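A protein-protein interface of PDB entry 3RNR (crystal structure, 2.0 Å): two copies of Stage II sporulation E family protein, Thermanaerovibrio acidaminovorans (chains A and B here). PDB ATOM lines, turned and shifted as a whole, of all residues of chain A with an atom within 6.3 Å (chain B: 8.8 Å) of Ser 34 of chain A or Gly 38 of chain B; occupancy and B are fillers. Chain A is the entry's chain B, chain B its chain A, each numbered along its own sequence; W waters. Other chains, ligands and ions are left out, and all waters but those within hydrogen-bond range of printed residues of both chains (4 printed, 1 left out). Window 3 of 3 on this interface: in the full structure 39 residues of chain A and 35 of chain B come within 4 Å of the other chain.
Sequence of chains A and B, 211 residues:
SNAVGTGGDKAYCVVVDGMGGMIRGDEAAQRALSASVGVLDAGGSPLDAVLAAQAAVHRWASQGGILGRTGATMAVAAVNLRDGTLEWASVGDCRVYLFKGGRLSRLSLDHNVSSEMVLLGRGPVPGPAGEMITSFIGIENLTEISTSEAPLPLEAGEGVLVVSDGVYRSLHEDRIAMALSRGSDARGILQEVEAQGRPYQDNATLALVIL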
ATOM      1  N   ALA A  29       5.275  22.653 -21.536  1.00  0.00           N
ATOM      2  CA  ALA A  29       5.800  23.122 -22.812  1.00  0.00           C
ATOM      3  C   ALA A  29       7.323  23.215 -22.762  1.00  0.00           C
ATOM      4  O   ALA A  29       7.992  22.870 -23.734  1.00  0.00           O
ATOM      5  CB  ALA A  29       5.197  24.463 -23.185  1.00  0.00           C
ATOM      6  N   GLN A  30       7.878  23.647 -21.626  1.00  0.00           N
ATOM      7  CA  GLN A  30       9.336  23.717 -21.506  1.00  0.00           C
ATOM      8  C   GLN A  30       9.994  22.359 -21.680  1.00  0.00           C
ATOM      9  O   GLN A  30      11.023  22.250 -22.337  1.00  0.00           O
ATOM     10  CB  GLN A  30       9.751  24.331 -20.165  1.00  0.00           C
ATOM     11  CG  GLN A  30       9.457  25.813 -20.087  1.00  0.00           C
ATOM     12  CD  GLN A  30       9.448  26.333 -18.675  1.00  0.00           C
ATOM     13  OE1 GLN A  30       9.716  25.594 -17.724  1.00  0.00           O
ATOM     14  NE2 GLN A  30       9.127  27.608 -18.525  1.00  0.00           N
ATOM     15  N   ARG A  31       9.419  21.321 -21.075  1.00  0.00           N
ATOM     16  CA  ARG A  31      10.005  19.989 -21.200  1.00  0.00           C
ATOM     17  C   ARG A  31       9.899  19.504 -22.623  1.00  0.00           C
ATOM     18  O   ARG A  31      10.817  18.876 -23.140  1.00  0.00           O
ATOM     19  CB  ARG A  31       9.308  18.976 -20.288  1.00  0.00           C
ATOM     20  CG  ARG A  31       9.931  18.897 -18.918  1.00  0.00           C
ATOM     21  CD  ARG A  31       9.261  19.838 -17.961  1.00  0.00           C
ATOM     22  NE  ARG A  31       9.931  19.805 -16.673  1.00  0.00           N
ATOM     23  CZ  ARG A  31      10.109  20.872 -15.907  1.00  0.00           C
ATOM     24  NH1 ARG A  31       9.640  22.053 -16.295  1.00  0.00           N
ATOM     25  NH2 ARG A  31      10.750  20.752 -14.751  1.00  0.00           N
ATOM     26  N   ALA A  32       8.769  19.782 -23.253  1.00  0.00           N
ATOM     27  CA  ALA A  32       8.573  19.353 -24.633  1.00  0.00           C
ATOM     28  C   ALA A  32       9.547  20.056 -25.580  1.00  0.00           C
ATOM     29  O   ALA A  32      10.155  19.437 -26.443  1.00  0.00           O
ATOM     30  CB  ALA A  32       7.108  19.588 -25.069  1.00  0.00           C
ATOM     31  N   LEU A  33       9.676  21.366 -25.427  1.00  0.00           N
ATOM     32  CA  LEU A  33      10.546  22.131 -26.302  1.00  0.00           C
ATOM     33  C   LEU A  33      11.996  21.666 -26.101  1.00  0.00           C
ATOM     34  O   LEU A  33      12.692  21.371 -27.054  1.00  0.00           O
ATOM     35  CB  LEU A  33      10.399  23.628 -25.984  1.00  0.00           C
ATOM     36  CG  LEU A  33      11.199  24.673 -26.771  1.00  0.00           C
ATOM     37  CD1 LEU A  33      12.716  24.586 -26.491  1.00  0.00           C
ATOM     38  CD2 LEU A  33      10.891  24.576 -28.264  1.00  0.00           C
ATOM     39  N   SER A  34      12.438  21.595 -24.849  1.00  0.00           N
ATOM     40  CA  SER A  34      13.826  21.237 -24.575  1.00  0.00           C
ATOM     41  C   SER A  34      14.156  19.830 -25.071  1.00  0.00           C
ATOM     42  O   SER A  34      15.207  19.609 -25.667  1.00  0.00           O
ATOM     43  CB  SER A  34      14.132  21.335 -23.081  1.00  0.00           C
ATOM     44  OG  SER A  34      15.495  21.031 -22.842  1.00  0.00           O
ATOM     45  N   ALA A  35      13.270  18.871 -24.822  1.00  0.00           N
ATOM     46  CA  ALA A  35      13.530  17.509 -25.282  1.00  0.00           C
ATOM     47  C   ALA A  35      13.558  17.434 -26.824  1.00  0.00           C
ATOM     48  O   ALA A  35      14.432  16.796 -27.413  1.00  0.00           O
ATOM     49  CB  ALA A  35      12.512  16.530 -24.701  1.00  0.00           C
ATOM     50  N   SER A  36      12.607  18.090 -27.476  1.00  0.00           N
ATOM     51  CA  SER A  36      12.542  18.027 -28.937  1.00  0.00           C
ATOM     52  C   SER A  36      13.766  18.657 -29.596  1.00  0.00           C
ATOM     53  O   SER A  36      14.287  18.123 -30.578  1.00  0.00           O
ATOM     54  CB  SER A  36      11.242  18.649 -29.472  1.00  0.00           C
ATOM     55  OG  SER A  36      11.150  20.024 -29.151  1.00  0.00           O
ATOM     56  N   VAL A  37      14.235  19.781 -29.054  1.00  0.00           N
ATOM     57  CA  VAL A  37      15.418  20.447 -29.607  1.00  0.00           C
ATOM     58  C   VAL A  37      16.698  19.628 -29.415  1.00  0.00           C
ATOM     59  O   VAL A  37      17.541  19.566 -30.305  1.00  0.00           O
ATOM     60  CB  VAL A  37      15.598  21.894 -29.036  1.00  0.00           C
ATOM     61  CG1 VAL A  37      16.992  22.438 -29.373  1.00  0.00           C
ATOM     62  CG2 VAL A  37      14.518  22.814 -29.599  1.00  0.00           C
ATOM     63  N   GLY A  38      16.845  18.988 -28.258  1.00  0.00           N
ATOM     64  CA  GLY A  38      17.969  18.092 -28.055  1.00  0.00           C
ATOM     65  C   GLY A  38      18.053  17.016 -29.128  1.00  0.00           C
ATOM     66  O   GLY A  38      19.129  16.714 -29.642  1.00  0.00           O
ATOM     67  N   VAL A  39      16.910  16.439 -29.479  1.00  0.00           N
ATOM     68  CA  VAL A  39      16.862  15.407 -30.515  1.00  0.00           C
ATOM     69  C   VAL A  39      17.172  16.007 -31.889  1.00  0.00           C
ATOM     70  O   VAL A  39      18.012  15.498 -32.625  1.00  0.00           O
ATOM     71  CB  VAL A  39      15.474  14.712 -30.559  1.00  0.00           C
ATOM     72  CG1 VAL A  39      15.298  13.941 -31.867  1.00  0.00           C
ATOM     73  CG2 VAL A  39      15.312  13.772 -29.360  1.00  0.00           C
ATOM     74  N   GLY B   7      10.787  32.042 -26.022  1.00  0.00           N
ATOM     75  CA  GLY B   7       9.971  31.456 -24.972  1.00  0.00           C
ATOM     76  C   GLY B   7      10.138  32.319 -23.731  1.00  0.00           C
ATOM     77  O   GLY B   7      11.161  32.989 -23.581  1.00  0.00           O
ATOM     78  N   TYR B  12      16.168  34.293 -28.169  1.00  0.00           N
ATOM     79  CA  TYR B  12      17.552  33.955 -27.881  1.00  0.00           C
ATOM     80  C   TYR B  12      18.216  33.328 -29.087  1.00  0.00           C
ATOM     81  O   TYR B  12      17.549  32.883 -30.013  1.00  0.00           O
ATOM     82  CB  TYR B  12      17.635  33.003 -26.669  1.00  0.00           C
ATOM     83  CG  TYR B  12      16.874  31.715 -26.919  1.00  0.00           C
ATOM     84  CD1 TYR B  12      17.456  30.671 -27.623  1.00  0.00           C
ATOM     85  CD2 TYR B  12      15.554  31.567 -26.496  1.00  0.00           C
ATOM     86  CE1 TYR B  12      16.746  29.488 -27.893  1.00  0.00           C
ATOM     87  CE2 TYR B  12      14.842  30.386 -26.747  1.00  0.00           C
ATOM     88  CZ  TYR B  12      15.442  29.357 -27.440  1.00  0.00           C
ATOM     89  OH  TYR B  12      14.737  28.186 -27.704  1.00  0.00           O
ATOM     90  N   VAL B  14      21.931  30.921 -30.108  1.00  0.00           N
ATOM     91  CA  VAL B  14      23.032  30.156 -29.588  1.00  0.00           C
ATOM     92  C   VAL B  14      23.798  29.542 -30.738  1.00  0.00           C
ATOM     93  O   VAL B  14      23.211  29.075 -31.719  1.00  0.00           O
ATOM     94  CB  VAL B  14      22.546  28.934 -28.776  1.00  0.00           C
ATOM     95  CG1 VAL B  14      23.677  28.404 -27.878  1.00  0.00           C
ATOM     96  CG2 VAL B  14      21.322  29.256 -27.978  1.00  0.00           C
ATOM     97  N   GLN B  30      26.525  19.040 -28.769  1.00  0.00           N
ATOM     98  CA  GLN B  30      25.093  18.739 -28.650  1.00  0.00           C
ATOM     99  C   GLN B  30      24.593  18.911 -27.220  1.00  0.00           C
ATOM    100  O   GLN B  30      23.521  19.473 -26.975  1.00  0.00           O
ATOM    101  CB  GLN B  30      24.804  17.312 -29.145  1.00  0.00           C
ATOM    102  CG  GLN B  30      24.994  17.154 -30.655  1.00  0.00           C
ATOM    103  CD  GLN B  30      25.162  15.704 -31.120  1.00  0.00           C
ATOM    104  OE1 GLN B  30      25.095  14.762 -30.329  1.00  0.00           O
ATOM    105  NE2 GLN B  30      25.393  15.531 -32.417  1.00  0.00           N
ATOM    106  N   ARG B  31      25.363  18.413 -26.264  1.00  0.00           N
ATOM    107  CA  ARG B  31      24.974  18.534 -24.862  1.00  0.00           C
ATOM    108  C   ARG B  31      24.981  19.981 -24.385  1.00  0.00           C
ATOM    109  O   ARG B  31      24.111  20.393 -23.615  1.00  0.00           O
ATOM    110  CB  ARG B  31      25.866  17.647 -23.996  1.00  0.00           C
ATOM    111  CG  ARG B  31      25.552  16.161 -24.248  1.00  0.00           C
ATOM    112  CD  ARG B  31      26.568  15.192 -23.650  1.00  0.00           C
ATOM    113  NE  ARG B  31      26.143  13.810 -23.897  1.00  0.00           N
ATOM    114  CZ  ARG B  31      25.299  13.129 -23.122  1.00  0.00           C
ATOM    115  NH1 ARG B  31      24.791  13.678 -22.028  1.00  0.00           N
ATOM    116  NH2 ARG B  31      24.964  11.883 -23.441  1.00  0.00           N
ATOM    117  N   ALA B  32      25.954  20.755 -24.858  1.00  0.00           N
ATOM    118  CA  ALA B  32      26.010  22.183 -24.534  1.00  0.00           C
ATOM    119  C   ALA B  32      24.805  22.925 -25.103  1.00  0.00           C
ATOM    120  O   ALA B  32      24.180  23.752 -24.438  1.00  0.00           O
ATOM    121  CB  ALA B  32      27.316  22.807 -25.076  1.00  0.00           C
ATOM    122  N   LEU B  33      24.493  22.656 -26.359  1.00  0.00           N
ATOM    123  CA  LEU B  33      23.397  23.365 -26.986  1.00  0.00           C
ATOM    124  C   LEU B  33      22.073  22.981 -26.332  1.00  0.00           C
ATOM    125  O   LEU B  33      21.232  23.836 -26.051  1.00  0.00           O
ATOM    126  CB  LEU B  33      23.371  23.118 -28.507  1.00  0.00           C
ATOM    127  CG  LEU B  33      22.257  23.951 -29.161  1.00  0.00           C
ATOM    128  CD1 LEU B  33      22.712  24.571 -30.459  1.00  0.00           C
ATOM    129  CD2 LEU B  33      20.976  23.101 -29.356  1.00  0.00           C
ATOM    130  N   SER B  34      21.888  21.689 -26.088  1.00  0.00           N
ATOM    131  CA  SER B  34      20.658  21.200 -25.463  1.00  0.00           C
ATOM    132  C   SER B  34      20.407  21.833 -24.102  1.00  0.00           C
ATOM    133  O   SER B  34      19.288  22.269 -23.791  1.00  0.00           O
ATOM    134  CB  SER B  34      20.712  19.678 -25.318  1.00  0.00           C
ATOM    135  OG  SER B  34      20.703  19.063 -26.588  1.00  0.00           O
ATOM    136  N   ALA B  35      21.444  21.876 -23.277  1.00  0.00           N
ATOM    137  CA  ALA B  35      21.320  22.489 -21.957  1.00  0.00           C
ATOM    138  C   ALA B  35      20.986  23.974 -22.074  1.00  0.00           C
ATOM    139  O   ALA B  35      20.149  24.502 -21.332  1.00  0.00           O
ATOM    140  CB  ALA B  35      22.610  22.295 -21.148  1.00  0.00           C
ATOM    141  N   SER B  36      21.648  24.653 -23.005  1.00  0.00           N
ATOM    142  CA  SER B  36      21.459  26.090 -23.171  1.00  0.00           C
ATOM    143  C   SER B  36      20.043  26.430 -23.580  1.00  0.00           C
ATOM    144  O   SER B  36      19.426  27.340 -23.034  1.00  0.00           O
ATOM    145  CB  SER B  36      22.425  26.629 -24.231  1.00  0.00           C
ATOM    146  OG  SER B  36      23.748  26.447 -23.785  1.00  0.00           O
ATOM    147  N   VAL B  37      19.534  25.705 -24.567  1.00  0.00           N
ATOM    148  CA  VAL B  37      18.187  25.968 -25.048  1.00  0.00           C
ATOM    149  C   VAL B  37      17.148  25.722 -23.953  1.00  0.00           C
ATOM    150  O   VAL B  37      16.227  26.511 -23.784  1.00  0.00           O
ATOM    151  CB  VAL B  37      17.873  25.166 -26.335  1.00  0.00           C
ATOM    152  CG1 VAL B  37      16.389  25.189 -26.632  1.00  0.00           C
ATOM    153  CG2 VAL B  37      18.668  25.748 -27.503  1.00  0.00           C
ATOM    154  N   GLY B  38      17.303  24.645 -23.192  1.00  0.00           N
ATOM    155  CA  GLY B  38      16.387  24.404 -22.088  1.00  0.00           C
ATOM    156  C   GLY B  38      16.381  25.575 -21.116  1.00  0.00           C
ATOM    157  O   GLY B  38      15.329  26.056 -20.714  1.00  0.00           O
ATOM    158  N   VAL B  39      17.564  26.038 -20.734  1.00  0.00           N
ATOM    159  CA  VAL B  39      17.665  27.173 -19.825  1.00  0.00           C
ATOM    160  C   VAL B  39      16.988  28.410 -20.410  1.00  0.00           C
ATOM    161  O   VAL B  39      16.195  29.071 -19.728  1.00  0.00           O
ATOM    162  CB  VAL B  39      19.141  27.486 -19.474  1.00  0.00           C
ATOM    163  CG1 VAL B  39      19.270  28.844 -18.793  1.00  0.00           C
ATOM    164  CG2 VAL B  39      19.728  26.388 -18.596  1.00  0.00           C
ATOM    165  N   LEU B  40      17.293  28.726 -21.670  1.00  0.00           N
ATOM    166  CA  LEU B  40      16.810  29.975 -22.279  1.00  0.00           C
ATOM    167  C   LEU B  40      15.303  29.974 -22.481  1.00  0.00           C
ATOM    168  O   LEU B  40      14.617  30.958 -22.190  1.00  0.00           O
ATOM    169  CB  LEU B  40      17.515  30.240 -23.611  1.00  0.00           C
ATOM    170  CG  LEU B  40      19.022  30.473 -23.420  1.00  0.00           C
ATOM    171  CD1 LEU B  40      19.787  30.124 -24.714  1.00  0.00           C
ATOM    172  CD2 LEU B  40      19.317  31.902 -22.931  1.00  0.00           C
ATOM    173  N   ASP B  41      14.787  28.862 -22.986  1.00  0.00           N
ATOM    174  CA  ASP B  41      13.356  28.734 -23.176  1.00  0.00           C
ATOM    175  C   ASP B  41      12.588  28.844 -21.851  1.00  0.00           C
ATOM    176  O   ASP B  41      11.459  29.323 -21.830  1.00  0.00           O
ATOM    177  CB  ASP B  41      13.029  27.413 -23.871  1.00  0.00           C
ATOM    178  CG  ASP B  41      11.533  27.212 -24.035  1.00  0.00           C
ATOM    179  OD1 ASP B  41      10.931  27.874 -24.899  1.00  0.00           O
ATOM    180  OD2 ASP B  41      10.964  26.401 -23.294  1.00  0.00           O
ATOM    181  N   ALA B  42      13.214  28.421 -20.754  1.00  0.00           N
ATOM    182  CA  ALA B  42      12.600  28.491 -19.423  1.00  0.00           C
ATOM    183  C   ALA B  42      12.773  29.859 -18.754  1.00  0.00           C
ATOM    184  O   ALA B  42      12.395  30.034 -17.599  1.00  0.00           O
ATOM    185  CB  ALA B  42      13.169  27.412 -18.514  1.00  0.00           C
ATOM    186  N   GLY B  43      13.392  30.807 -19.445  1.00  0.00           N
ATOM    187  CA  GLY B  43      13.498  32.160 -18.915  1.00  0.00           C
ATOM    188  C   GLY B  43      14.857  32.521 -18.344  1.00  0.00           C
ATOM    189  O   GLY B  43      15.033  33.592 -17.777  1.00  0.00           O
ATOM    190  N   GLY B  44      15.837  31.641 -18.507  1.00  0.00           N
ATOM    191  CA  GLY B  44      17.152  31.896 -17.950  1.00  0.00           C
ATOM    192  C   GLY B  44      17.981  32.833 -18.818  1.00  0.00           C
ATOM    193  O   GLY B  44      17.632  33.126 -19.959  1.00  0.00           O
ATOM    194  N   SER B  45      19.074  33.321 -18.254  1.00  0.00           N
ATOM    195  CA  SER B  45      19.988  34.223 -18.942  1.00  0.00           C
ATOM    196  C   SER B  45      21.051  33.479 -19.760  1.00  0.00           C
ATOM    197  O   SER B  45      21.276  32.293 -19.570  1.00  0.00           O
ATOM    198  CB  SER B  45      20.687  35.096 -17.910  1.00  0.00           C
ATOM    199  OG  SER B  45      21.542  34.295 -17.117  1.00  0.00           O
ATOM    200  N   ASP B  48      23.436  31.951 -17.328  1.00  0.00           N
ATOM    201  CA  ASP B  48      22.825  30.707 -16.812  1.00  0.00           C
ATOM    202  C   ASP B  48      23.041  29.549 -17.780  1.00  0.00           C
ATOM    203  O   ASP B  48      23.311  28.416 -17.371  1.00  0.00           O
ATOM    204  CB  ASP B  48      21.304  30.839 -16.646  1.00  0.00           C
ATOM    205  CG  ASP B  48      20.891  31.824 -15.563  1.00  0.00           C
ATOM    206  OD1 ASP B  48      21.730  32.196 -14.731  1.00  0.00           O
ATOM    207  OD2 ASP B  48      19.704  32.225 -15.565  1.00  0.00           O
ATOM    208  N   ALA B  49      22.856  29.828 -19.071  1.00  0.00           N
ATOM    209  CA  ALA B  49      22.913  28.797 -20.107  1.00  0.00           C
ATOM    210  C   ALA B  49      24.323  28.234 -20.247  1.00  0.00           C
ATOM    211  O   ALA B  49      24.525  27.017 -20.370  1.00  0.00           O
ATOM    212  CB  ALA B  49      22.429  29.390 -21.466  1.00  0.00           C
ATOM    213  N   ALA B  52      25.029  26.021 -17.232  1.00  0.00           N
ATOM    214  CA  ALA B  52      24.291  24.764 -17.318  1.00  0.00           C
ATOM    215  C   ALA B  52      24.942  23.826 -18.336  1.00  0.00           C
ATOM    216  O   ALA B  52      25.061  22.618 -18.107  1.00  0.00           O
ATOM    217  CB  ALA B  52      22.830  25.036 -17.691  1.00  0.00           C
HETATM  218  O   HOH W   1      21.519  18.016 -29.078  1.00  0.00           O
HETATM  219  O   HOH W   2      17.488  20.467 -24.222  1.00  0.00           O
HETATM  220  O   HOH W   3       8.940  29.185 -21.004  1.00  0.00           O
HETATM  221  O   HOH W   4       8.295  26.346 -23.416  1.00  0.00           O
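The side-chain hydroxyl (OG) of Ser 36 of chain A lies within hydrogen-bond range of the backbone carbonyl oxygen (O) of Leu 33 of chain A (2.9 Å).
The backbone carbonyl oxygen (O) of Gln 30 of chain B sits at hydrogen-bond distance from the side-chain hydroxyl (OG) of Ser 34 of chain B (2.9 Å).
Among the printed residues, merely in contact across the chains: Gly 38 of chain A with Ser 34 of chain B (3.3 Å), Ser 34 of chain A with Gly 38 of chain B (3.6 Å), Gln 30 of chain A with Asp 41 of chain B (3.6 Å), Gln 30 of chain A with Ala 42 of chain B (3.7 Å), Leu 33 of chain A with Asp 41 of chain B (3.7 Å), Leu 33 of chain A with Val 37 of chain B (3.7 Å) and Val 37 of chain A with Val 37 of chain B (3.9 Å).
Of the printed residues of chain B, Leu 33 of chain A touches Val 37 and Asp 41.
Printed residues of chain B within 4 Å of Ser 34 of chain A: Gly 38 (3.6 Å).
No residue of chain B comes within 4 Å of Ala 35 of chain A.
Printed residues of chain B within 4 Å of Gly 38 of chain A: Ser 34 (3.3 Å).
The nearest printed residue of chain A that does not touch Gly 38 of chain B is Leu 33 of chain A (5.7 Å).
Among the printed residues, 7 pairs touch across the chains.
Among the printed residues, no Asp or Glu carboxylate lies within 4 Å of a Lys or Arg side-chain nitrogen of the other chain.
Leu 33 of chain A touches Val 37 of chain B, but with the chains exchanged Val 37 of chain A does not touch Leu 33 of chain B (4.04 Å).
Ser 34 of chain A touches Gly 38 of chain B, and with the chains exchanged Gly 38 of chain A touches Ser 34 of chain B.
Val 37 of chain B touches its own counterpart, Val 37 of chain A.
Positions printed for both chains: 30, 31, 32, 33, 34, 35, 36, 37, 38 and 39.
Of the 7 pairs that touch across the chains among the printed residues, 3 have their exchanged pair printed and touching as well.
Water W2 bridges the side-chain hydroxyl (OG) of Ser 34 of chain A (2.5 Å) and the backbone carbonyl oxygen (O) of Ser 34 of chain B (2.6 Å).
Water W3 lies within hydrogen-bond range of the backbone carbonyl oxygen (O) of Asp 41 of chain B (2.7 Å) and the side-chain amide nitrogen (NE2) of Gln 30 of chain A (2.9 Å).
Water W4 lies within hydrogen-bond range of the side-chain carboxylate of Asp 41 of chain B and the backbone NH of Gln 30 of chain A.
Water W1 lies within hydrogen-bond range of the backbone carbonyl oxygen of Gly 38 of chain A (2.8 Å), the side-chain hydroxyl of Ser 34 of chain B (2.8 Å) and the backbone carbonyl oxygen of Gln 30 of chain B (3.2 Å).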
